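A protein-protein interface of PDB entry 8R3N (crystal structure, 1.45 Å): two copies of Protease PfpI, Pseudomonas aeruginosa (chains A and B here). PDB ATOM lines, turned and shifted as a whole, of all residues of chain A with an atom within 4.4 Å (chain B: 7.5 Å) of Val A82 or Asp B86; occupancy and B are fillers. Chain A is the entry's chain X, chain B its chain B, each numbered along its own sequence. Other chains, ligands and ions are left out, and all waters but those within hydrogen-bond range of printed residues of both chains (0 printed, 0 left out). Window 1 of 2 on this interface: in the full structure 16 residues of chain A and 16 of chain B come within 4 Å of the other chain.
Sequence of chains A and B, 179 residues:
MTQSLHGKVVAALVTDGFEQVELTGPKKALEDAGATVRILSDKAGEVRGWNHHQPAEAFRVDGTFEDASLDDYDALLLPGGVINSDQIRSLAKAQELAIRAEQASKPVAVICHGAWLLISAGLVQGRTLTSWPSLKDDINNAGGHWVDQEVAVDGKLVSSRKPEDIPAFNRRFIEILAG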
ATOM      1  N   GLY A  80      15.484  -0.651  14.273  1.00  0.00           N
ATOM      2  CA  GLY A  80      15.414  -0.430  15.700  1.00  0.00           C
ATOM      3  C   GLY A  80      14.733  -1.546  16.459  1.00  0.00           C
ATOM      4  O   GLY A  80      15.019  -2.726  16.247  1.00  0.00           O
ATOM      5  N   GLY A  81      13.826  -1.182  17.358  1.00  0.00           N
ATOM      6  CA  GLY A  81      13.427  -2.113  18.387  1.00  0.00           C
ATOM      7  C   GLY A  81      14.362  -1.878  19.542  1.00  0.00           C
ATOM      8  O   GLY A  81      15.567  -2.118  19.410  1.00  0.00           O
ATOM      9  N   VAL A  82      13.833  -1.370  20.662  1.00  0.00           N
ATOM     10  CA  VAL A  82      14.678  -1.109  21.826  1.00  0.00           C
ATOM     11  C   VAL A  82      15.416  -2.377  22.276  1.00  0.00           C
ATOM     12  O   VAL A  82      16.592  -2.324  22.661  1.00  0.00           O
ATOM     13  CB  VAL A  82      13.876  -0.407  22.945  1.00  0.00           C
ATOM     14  CG1 VAL A  82      12.773  -1.313  23.464  1.00  0.00           C
ATOM     15  CG2 VAL A  82      14.821  -0.025  24.078  1.00  0.00           C
ATOM     16  N   ILE A  83      14.756  -3.539  22.207  1.00  0.00           N
ATOM     17  CA  ILE A  83      15.365  -4.776  22.692  1.00  0.00           C
ATOM     18  C   ILE A  83      16.526  -5.187  21.797  1.00  0.00           C
ATOM     19  O   ILE A  83      17.633  -5.455  22.279  1.00  0.00           O
ATOM     20  CB  ILE A  83      14.317  -5.896  22.831  1.00  0.00           C
ATOM     21  CG1 ILE A  83      13.342  -5.590  23.977  1.00  0.00           C
ATOM     22  CG2 ILE A  83      15.006  -7.256  23.048  1.00  0.00           C
ATOM     23  CD1 ILE A  83      12.146  -6.534  24.011  1.00  0.00           C
ATOM     24  N   ASN A  84      16.293  -5.232  20.484  1.00  0.00           N
ATOM     25  CA  ASN A  84      17.363  -5.551  19.541  1.00  0.00           C
ATOM     26  C   ASN A  84      18.492  -4.543  19.657  1.00  0.00           C
ATOM     27  O   ASN A  84      19.671  -4.913  19.693  1.00  0.00           O
ATOM     28  CB  ASN A  84      16.810  -5.516  18.118  1.00  0.00           C
ATOM     29  CG  ASN A  84      17.902  -5.317  17.065  1.00  0.00           C
ATOM     30  OD1 ASN A  84      18.834  -6.109  16.982  1.00  0.00           O
ATOM     31  ND2 ASN A  84      17.772  -4.253  16.238  1.00  0.00           N
ATOM     32  N   SER A  85      18.140  -3.257  19.727  1.00  0.00           N
ATOM     33  CA  SER A  85      19.152  -2.212  19.676  1.00  0.00           C
ATOM     34  C   SER A  85      20.044  -2.265  20.907  1.00  0.00           C
ATOM     35  O   SER A  85      21.253  -2.024  20.820  1.00  0.00           O
ATOM     36  CB  SER A  85      18.487  -0.839  19.523  1.00  0.00           C
ATOM     37  OG  SER A  85      17.630  -0.828  18.376  1.00  0.00           O
ATOM     38  N   ASP A  86      19.450  -2.539  22.069  1.00  0.00           N
ATOM     39  CA  ASP A  86      20.234  -2.672  23.282  1.00  0.00           C
ATOM     40  C   ASP A  86      21.146  -3.893  23.244  1.00  0.00           C
ATOM     41  O   ASP A  86      22.253  -3.841  23.791  1.00  0.00           O
ATOM     42  CB  ASP A  86      19.287  -2.677  24.482  1.00  0.00           C
ATOM     43  CG  ASP A  86      20.013  -2.869  25.782  1.00  0.00           C
ATOM     44  OD1 ASP A  86      20.583  -1.881  26.293  1.00  0.00           O
ATOM     45  OD2 ASP A  86      20.011  -4.016  26.274  1.00  0.00           O
ATOM     46  N   HIS A 113      15.776   3.186  17.651  1.00  0.00           N
ATOM     47  CA  HIS A 113      16.816   2.932  18.686  1.00  0.00           C
ATOM     48  C   HIS A 113      18.100   2.363  18.072  1.00  0.00           C
ATOM     49  O   HIS A 113      19.060   2.229  18.770  1.00  0.00           O
ATOM     50  CB  HIS A 113      16.280   1.965  19.747  1.00  0.00           C
ATOM     51  CG  HIS A 113      15.169   2.469  20.599  1.00  0.00           C
ATOM     52  ND1 HIS A 113      13.854   2.401  20.212  1.00  0.00           N
ATOM     53  CD2 HIS A 113      15.164   2.974  21.846  1.00  0.00           C
ATOM     54  CE1 HIS A 113      13.089   2.873  21.164  1.00  0.00           C
ATOM     55  NE2 HIS A 113      13.870   3.235  22.172  1.00  0.00           N
ATOM     56  N   TRP A 116      22.326   2.994  18.588  1.00  0.00           N
ATOM     57  CA  TRP A 116      23.210   2.607  19.682  1.00  0.00           C
ATOM     58  C   TRP A 116      24.400   1.791  19.188  1.00  0.00           C
ATOM     59  O   TRP A 116      25.505   1.895  19.739  1.00  0.00           O
ATOM     60  CB  TRP A 116      22.432   1.799  20.706  1.00  0.00           C
ATOM     61  CG  TRP A 116      21.725   2.634  21.751  1.00  0.00           C
ATOM     62  CD1 TRP A 116      22.189   3.774  22.358  1.00  0.00           C
ATOM     63  CD2 TRP A 116      20.462   2.345  22.341  1.00  0.00           C
ATOM     64  NE1 TRP A 116      21.273   4.214  23.285  1.00  0.00           N
ATOM     65  CE2 TRP A 116      20.201   3.358  23.288  1.00  0.00           C
ATOM     66  CE3 TRP A 116      19.514   1.338  22.151  1.00  0.00           C
ATOM     67  CZ2 TRP A 116      19.032   3.384  24.047  1.00  0.00           C
ATOM     68  CZ3 TRP A 116      18.353   1.366  22.912  1.00  0.00           C
ATOM     69  CH2 TRP A 116      18.119   2.384  23.837  1.00  0.00           C
ATOM     70  N   SER A 134      14.572   9.218  22.730  1.00  0.00           N
ATOM     71  CA  SER A 134      15.205   8.625  23.924  1.00  0.00           C
ATOM     72  C   SER A 134      16.723   8.537  23.734  1.00  0.00           C
ATOM     73  O   SER A 134      17.421   8.541  24.732  1.00  0.00           O
ATOM     74  CB  SER A 134      14.607   7.285  24.247  1.00  0.00           C
ATOM     75  OG  SER A 134      15.016   6.287  23.332  1.00  0.00           O
ATOM     76  N   THR B  15       7.936   2.808  35.132  1.00  0.00           N
ATOM     77  CA  THR B  15       6.914   2.903  34.092  1.00  0.00           C
ATOM     78  C   THR B  15       6.634   1.490  33.596  1.00  0.00           C
ATOM     79  O   THR B  15       7.299   0.540  34.000  1.00  0.00           O
ATOM     80  CB  THR B  15       7.352   3.830  32.942  1.00  0.00           C
ATOM     81  OG1 THR B  15       8.439   3.251  32.203  1.00  0.00           O
ATOM     82  CG2 THR B  15       7.786   5.186  33.474  1.00  0.00           C
ATOM     83  N   GLY B  17       6.842  -1.861  31.838  1.00  0.00           N
ATOM     84  CA  GLY B  17       7.986  -2.543  31.277  1.00  0.00           C
ATOM     85  C   GLY B  17       9.200  -2.580  32.169  1.00  0.00           C
ATOM     86  O   GLY B  17      10.309  -2.819  31.665  1.00  0.00           O
ATOM     87  N   GLY B  80      15.245  -1.519  36.836  1.00  0.00           N
ATOM     88  CA  GLY B  80      15.538  -1.466  35.420  1.00  0.00           C
ATOM     89  C   GLY B  80      14.425  -1.983  34.540  1.00  0.00           C
ATOM     90  O   GLY B  80      13.243  -1.704  34.763  1.00  0.00           O
ATOM     91  N   GLY B  81      14.815  -2.755  33.537  1.00  0.00           N
ATOM     92  CA  GLY B  81      13.952  -3.135  32.434  1.00  0.00           C
ATOM     93  C   GLY B  81      14.227  -2.250  31.231  1.00  0.00           C
ATOM     94  O   GLY B  81      14.077  -1.027  31.309  1.00  0.00           O
ATOM     95  N   VAL B  82      14.647  -2.835  30.110  1.00  0.00           N
ATOM     96  CA  VAL B  82      15.027  -2.005  28.966  1.00  0.00           C
ATOM     97  C   VAL B  82      13.862  -1.135  28.481  1.00  0.00           C
ATOM     98  O   VAL B  82      14.052   0.040  28.135  1.00  0.00           O
ATOM     99  CB  VAL B  82      15.662  -2.855  27.842  1.00  0.00           C
ATOM    100  CG1 VAL B  82      14.612  -3.621  27.043  1.00  0.00           C
ATOM    101  CG2 VAL B  82      16.502  -1.976  26.928  1.00  0.00           C
ATOM    102  N   ILE B  83      12.637  -1.669  28.485  1.00  0.00           N
ATOM    103  CA  ILE B  83      11.491  -0.879  28.038  1.00  0.00           C
ATOM    104  C   ILE B  83      11.210   0.270  29.004  1.00  0.00           C
ATOM    105  O   ILE B  83      11.093   1.425  28.593  1.00  0.00           O
ATOM    106  CB  ILE B  83      10.260  -1.774  27.816  1.00  0.00           C
ATOM    107  CG1 ILE B  83      10.437  -2.618  26.553  1.00  0.00           C
ATOM    108  CG2 ILE B  83       9.000  -0.946  27.724  1.00  0.00           C
ATOM    109  CD1 ILE B  83       9.314  -3.590  26.318  1.00  0.00           C
ATOM    110  N   ASN B  84      11.123  -0.026  30.306  1.00  0.00           N
ATOM    111  CA  ASN B  84      10.870   1.029  31.286  1.00  0.00           C
ATOM    112  C   ASN B  84      11.988   2.062  31.288  1.00  0.00           C
ATOM    113  O   ASN B  84      11.736   3.273  31.248  1.00  0.00           O
ATOM    114  CB  ASN B  84      10.728   0.419  32.687  1.00  0.00           C
ATOM    115  CG  ASN B  84      11.073   1.408  33.800  1.00  0.00           C
ATOM    116  OD1 ASN B  84      10.418   2.427  33.942  1.00  0.00           O
ATOM    117  ND2 ASN B  84      12.107   1.101  34.590  1.00  0.00           N
ATOM    118  N   SER B  85      13.235   1.601  31.383  1.00  0.00           N
ATOM    119  CA  SER B  85      14.357   2.526  31.548  1.00  0.00           C
ATOM    120  C   SER B  85      14.463   3.484  30.373  1.00  0.00           C
ATOM    121  O   SER B  85      14.806   4.659  30.546  1.00  0.00           O
ATOM    122  CB  SER B  85      15.658   1.737  31.722  1.00  0.00           C
ATOM    123  OG  SER B  85      15.578   0.865  32.853  1.00  0.00           O
ATOM    124  N   ASP B  86      14.140   3.002  29.170  1.00  0.00           N
ATOM    125  CA  ASP B  86      14.171   3.830  27.970  1.00  0.00           C
ATOM    126  C   ASP B  86      13.047   4.866  27.971  1.00  0.00           C
ATOM    127  O   ASP B  86      13.250   6.010  27.546  1.00  0.00           O
ATOM    128  CB  ASP B  86      14.102   2.898  26.760  1.00  0.00           C
ATOM    129  CG  ASP B  86      14.017   3.642  25.432  1.00  0.00           C
ATOM    130  OD1 ASP B  86      15.032   4.219  24.988  1.00  0.00           O
ATOM    131  OD2 ASP B  86      12.920   3.612  24.831  1.00  0.00           O
ATOM    132  N   GLN B  87      11.864   4.480  28.449  1.00  0.00           N
ATOM    133  CA  GLN B  87      10.725   5.391  28.525  1.00  0.00           C
ATOM    134  C   GLN B  87      10.946   6.451  29.603  1.00  0.00           C
ATOM    135  O   GLN B  87      10.749   7.650  29.361  1.00  0.00           O
ATOM    136  CB  GLN B  87       9.476   4.580  28.899  1.00  0.00           C
ATOM    137  CG  GLN B  87       8.786   3.882  27.743  1.00  0.00           C
ATOM    138  CD  GLN B  87       7.831   2.752  28.177  1.00  0.00           C
ATOM    139  OE1 GLN B  87       7.215   2.096  27.318  1.00  0.00           O
ATOM    140  NE2 GLN B  87       7.646   2.565  29.505  1.00  0.00           N
ATOM    141  N   ILE B  88      11.333   6.017  30.812  1.00  0.00           N
ATOM    142  CA  ILE B  88      11.329   6.901  31.979  1.00  0.00           C
ATOM    143  C   ILE B  88      12.388   7.993  31.871  1.00  0.00           C
ATOM    144  O   ILE B  88      12.250   9.062  32.480  1.00  0.00           O
ATOM    145  CB  ILE B  88      11.473   6.094  33.294  1.00  0.00           C
ATOM    146  CG1 ILE B  88      10.990   6.942  34.484  1.00  0.00           C
ATOM    147  CG2 ILE B  88      12.932   5.656  33.512  1.00  0.00           C
ATOM    148  CD1 ILE B  88      11.015   6.217  35.845  1.00  0.00           C
ATOM    149  N   ARG B  89      13.458   7.757  31.104  1.00  0.00           N
ATOM    150  CA  ARG B  89      14.585   8.687  31.097  1.00  0.00           C
ATOM    151  C   ARG B  89      14.204  10.064  30.550  1.00  0.00           C
ATOM    152  O   ARG B  89      14.856  11.058  30.882  1.00  0.00           O
ATOM    153  CB  ARG B  89      15.763   8.093  30.316  1.00  0.00           C
ATOM    154  CG  ARG B  89      15.573   8.135  28.799  1.00  0.00           C
ATOM    155  CD  ARG B  89      16.728   7.476  28.098  1.00  0.00           C
ATOM    156  NE  ARG B  89      17.979   8.211  28.245  1.00  0.00           N
ATOM    157  CZ  ARG B  89      19.097   7.832  27.639  1.00  0.00           C
ATOM    158  NH1 ARG B  89      19.115   6.784  26.844  1.00  0.00           N
ATOM    159  NH2 ARG B  89      20.211   8.537  27.821  1.00  0.00           N
ATOM    160  N   SER B  90      13.179  10.142  29.710  1.00  0.00           N
ATOM    161  CA  SER B  90      12.797  11.393  29.065  1.00  0.00           C
ATOM    162  C   SER B  90      11.789  12.206  29.865  1.00  0.00           C
ATOM    163  O   SER B  90      11.521  13.358  29.504  1.00  0.00           O
ATOM    164  CB  SER B  90      12.193  11.103  27.696  1.00  0.00           C
ATOM    165  OG  SER B  90      11.036  10.297  27.841  1.00  0.00           O
ATOM    166  N   LEU B  91      11.216  11.637  30.921  1.00  0.00           N
ATOM    167  CA  LEU B  91      10.161  12.305  31.675  1.00  0.00           C
ATOM    168  C   LEU B  91      10.786  13.322  32.620  1.00  0.00           C
ATOM    169  O   LEU B  91      11.488  12.952  33.567  1.00  0.00           O
ATOM    170  CB  LEU B  91       9.349  11.269  32.447  1.00  0.00           C
ATOM    171  CG  LEU B  91       8.725  10.166  31.586  1.00  0.00           C
ATOM    172  CD1 LEU B  91       7.910   9.180  32.431  1.00  0.00           C
ATOM    173  CD2 LEU B  91       7.869  10.762  30.466  1.00  0.00           C
ATOM    174  N   HIS B 113      19.353  -1.531  33.686  1.00  0.00           N
ATOM    175  CA  HIS B 113      19.220  -0.484  32.681  1.00  0.00           C
ATOM    176  C   HIS B 113      18.786   0.849  33.294  1.00  0.00           C
ATOM    177  O   HIS B 113      18.661   1.845  32.577  1.00  0.00           O
ATOM    178  CB  HIS B 113      18.185  -0.892  31.624  1.00  0.00           C
ATOM    179  CG  HIS B 113      18.657  -1.956  30.679  1.00  0.00           C
ATOM    180  ND1 HIS B 113      18.487  -3.295  30.945  1.00  0.00           N
ATOM    181  CD2 HIS B 113      19.269  -1.888  29.473  1.00  0.00           C
ATOM    182  CE1 HIS B 113      18.997  -4.014  29.959  1.00  0.00           C
ATOM    183  NE2 HIS B 113      19.462  -3.181  29.047  1.00  0.00           N
ATOM    184  N   GLY B 114      18.547   0.897  34.604  1.00  0.00           N
ATOM    185  CA  GLY B 114      17.860   2.030  35.189  1.00  0.00           C
ATOM    186  C   GLY B 114      18.641   3.329  35.209  1.00  0.00           C
ATOM    187  O   GLY B 114      18.050   4.362  35.546  1.00  0.00           O
ATOM    188  N   TRP B 116      19.744   5.089  32.825  1.00  0.00           N
ATOM    189  CA  TRP B 116      19.509   5.996  31.710  1.00  0.00           C
ATOM    190  C   TRP B 116      18.867   7.289  32.191  1.00  0.00           C
ATOM    191  O   TRP B 116      19.172   8.370  31.678  1.00  0.00           O
ATOM    192  CB  TRP B 116      18.640   5.324  30.643  1.00  0.00           C
ATOM    193  CG  TRP B 116      19.419   4.624  29.568  1.00  0.00           C
ATOM    194  CD1 TRP B 116      20.629   4.993  29.033  1.00  0.00           C
ATOM    195  CD2 TRP B 116      19.027   3.430  28.881  1.00  0.00           C
ATOM    196  NE1 TRP B 116      21.013   4.087  28.057  1.00  0.00           N
ATOM    197  CE2 TRP B 116      20.046   3.122  27.950  1.00  0.00           C
ATOM    198  CE3 TRP B 116      17.915   2.583  28.969  1.00  0.00           C
ATOM    199  CZ2 TRP B 116      19.982   2.007  27.123  1.00  0.00           C
ATOM    200  CZ3 TRP B 116      17.851   1.480  28.137  1.00  0.00           C
ATOM    201  CH2 TRP B 116      18.873   1.209  27.219  1.00  0.00           C
ATOM    202  N   LEU B 117      17.986   7.195  33.192  1.00  0.00           N
ATOM    203  CA  LEU B 117      17.335   8.384  33.729  1.00  0.00           C
ATOM    204  C   LEU B 117      18.348   9.315  34.387  1.00  0.00           C
ATOM    205  O   LEU B 117      18.260  10.542  34.254  1.00  0.00           O
ATOM    206  CB  LEU B 117      16.288   7.965  34.759  1.00  0.00           C
ATOM    207  CG  LEU B 117      15.667   9.099  35.594  1.00  0.00           C
ATOM    208  CD1 LEU B 117      14.768   9.970  34.729  1.00  0.00           C
ATOM    209  CD2 LEU B 117      14.923   8.540  36.795  1.00  0.00           C
ATOM    210  N   SER B 120      20.151  11.187  31.555  1.00  0.00           N
ATOM    211  CA  SER B 120      19.344  12.257  30.984  1.00  0.00           C
ATOM    212  C   SER B 120      19.095  13.389  31.969  1.00  0.00           C
ATOM    213  O   SER B 120      18.867  14.525  31.542  1.00  0.00           O
ATOM    214  CB  SER B 120      18.044  11.677  30.425  1.00  0.00           C
ATOM    215  OG  SER B 120      18.347  10.862  29.300  1.00  0.00           O
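Val A82 touches its own counterpart, Val B82. Ile A83 touches Val B82, but with the chains exchanged Val A82 does not touch Ile B83 (4.1 Å). Asp A86 touches Trp B116, and with the chains exchanged Trp A116 touches Asp B86. Trp A116 touches its own counterpart, Trp B116. Positions printed for both chains: 80, 81, 82, 83, 84, 85, 86, 113 and 116. Of the 11 pairs that touch across the chains among the printed residues, 8 have their exchanged pair printed and touching as well.
Along chain B the printed residues that touch a printed residue of chain A span positions 82 to 116. Printed residues of chain A that touch a printed residue of chain B: Val A82, Ile A83, Asp A86, His A113, Trp A116 and Ser A134. Among the printed residues, 11 pairs touch across the chains. Among the printed residues, no Asp or Glu carboxylate lies within 4 Å of a Lys or Arg side-chain nitrogen of the other chain.
Of the printed residues of chain B, Val A82 touches Val B82 and Asp B86. Printed residues of chain A within 4 Å of Asp B86: Val A82 (3.99 Å), His A113 (2.8 Å), Trp A116 (3.8 Å) and Ser A134 (2.6 Å). No residue of chain B comes within 4 Å of Gly A81. Printed residues of chain A within 4 Å of Trp B116: Asp A86 (3.7 Å) and Trp A116 (3.5 Å). Printed residues of chain B within 4 Å of Trp A116: Asp B86 and Trp B116. Ser B85 touches none of the printed residues of chain A. The nearest printed residue of chain A that does not touch Asp B86 is Gly A81 (7.8 Å).
The side-chain hydroxyl (OG) of Ser A134 is in hydrogen-bond range of the side-chain carboxylate (OD1) of Asp B86, 2.6 Å away. A ring nitrogen (NE2) of His B113 is in hydrogen-bond range of the side-chain carboxylate (OD2) of Asp A86, at 2.9 Å. The guanidinium group (NH1) of Arg B89 lies within hydrogen-bond range of the backbone carbonyl oxygen (O) of Ser A134, 3.2 Å away. The side-chain carboxylate (OD2) of Asp B86 lies within hydrogen-bond range of a ring nitrogen (NE2) of His A113.
The side-chain hydroxyl (OG) of Ser A134 is in hydrogen-bond range of a ring nitrogen (NE2) of His A113 (3.5 Å). The backbone carbonyl oxygen (O) of His A113 lies close to the side-chain hydroxyl (OG) of Ser A85, 3.4 Å away. The backbone carbonyl oxygen (O) of His B113 lies close to the side-chain hydroxyl (OG) of Ser B85 (3.2 Å). OG of Ser B120 sits at hydrogen-bond distance from NE of Arg B89, 2.9 Å away.
Among the printed residues, merely in contact across the chains: Val A82 with Val B82, Val A82 with Asp B86, Ile A83 with Val B82, Asp A86 with Val B82, Asp A86 with Trp B116, Trp A116 with Asp B86 and Trp A116 with Trp B116.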
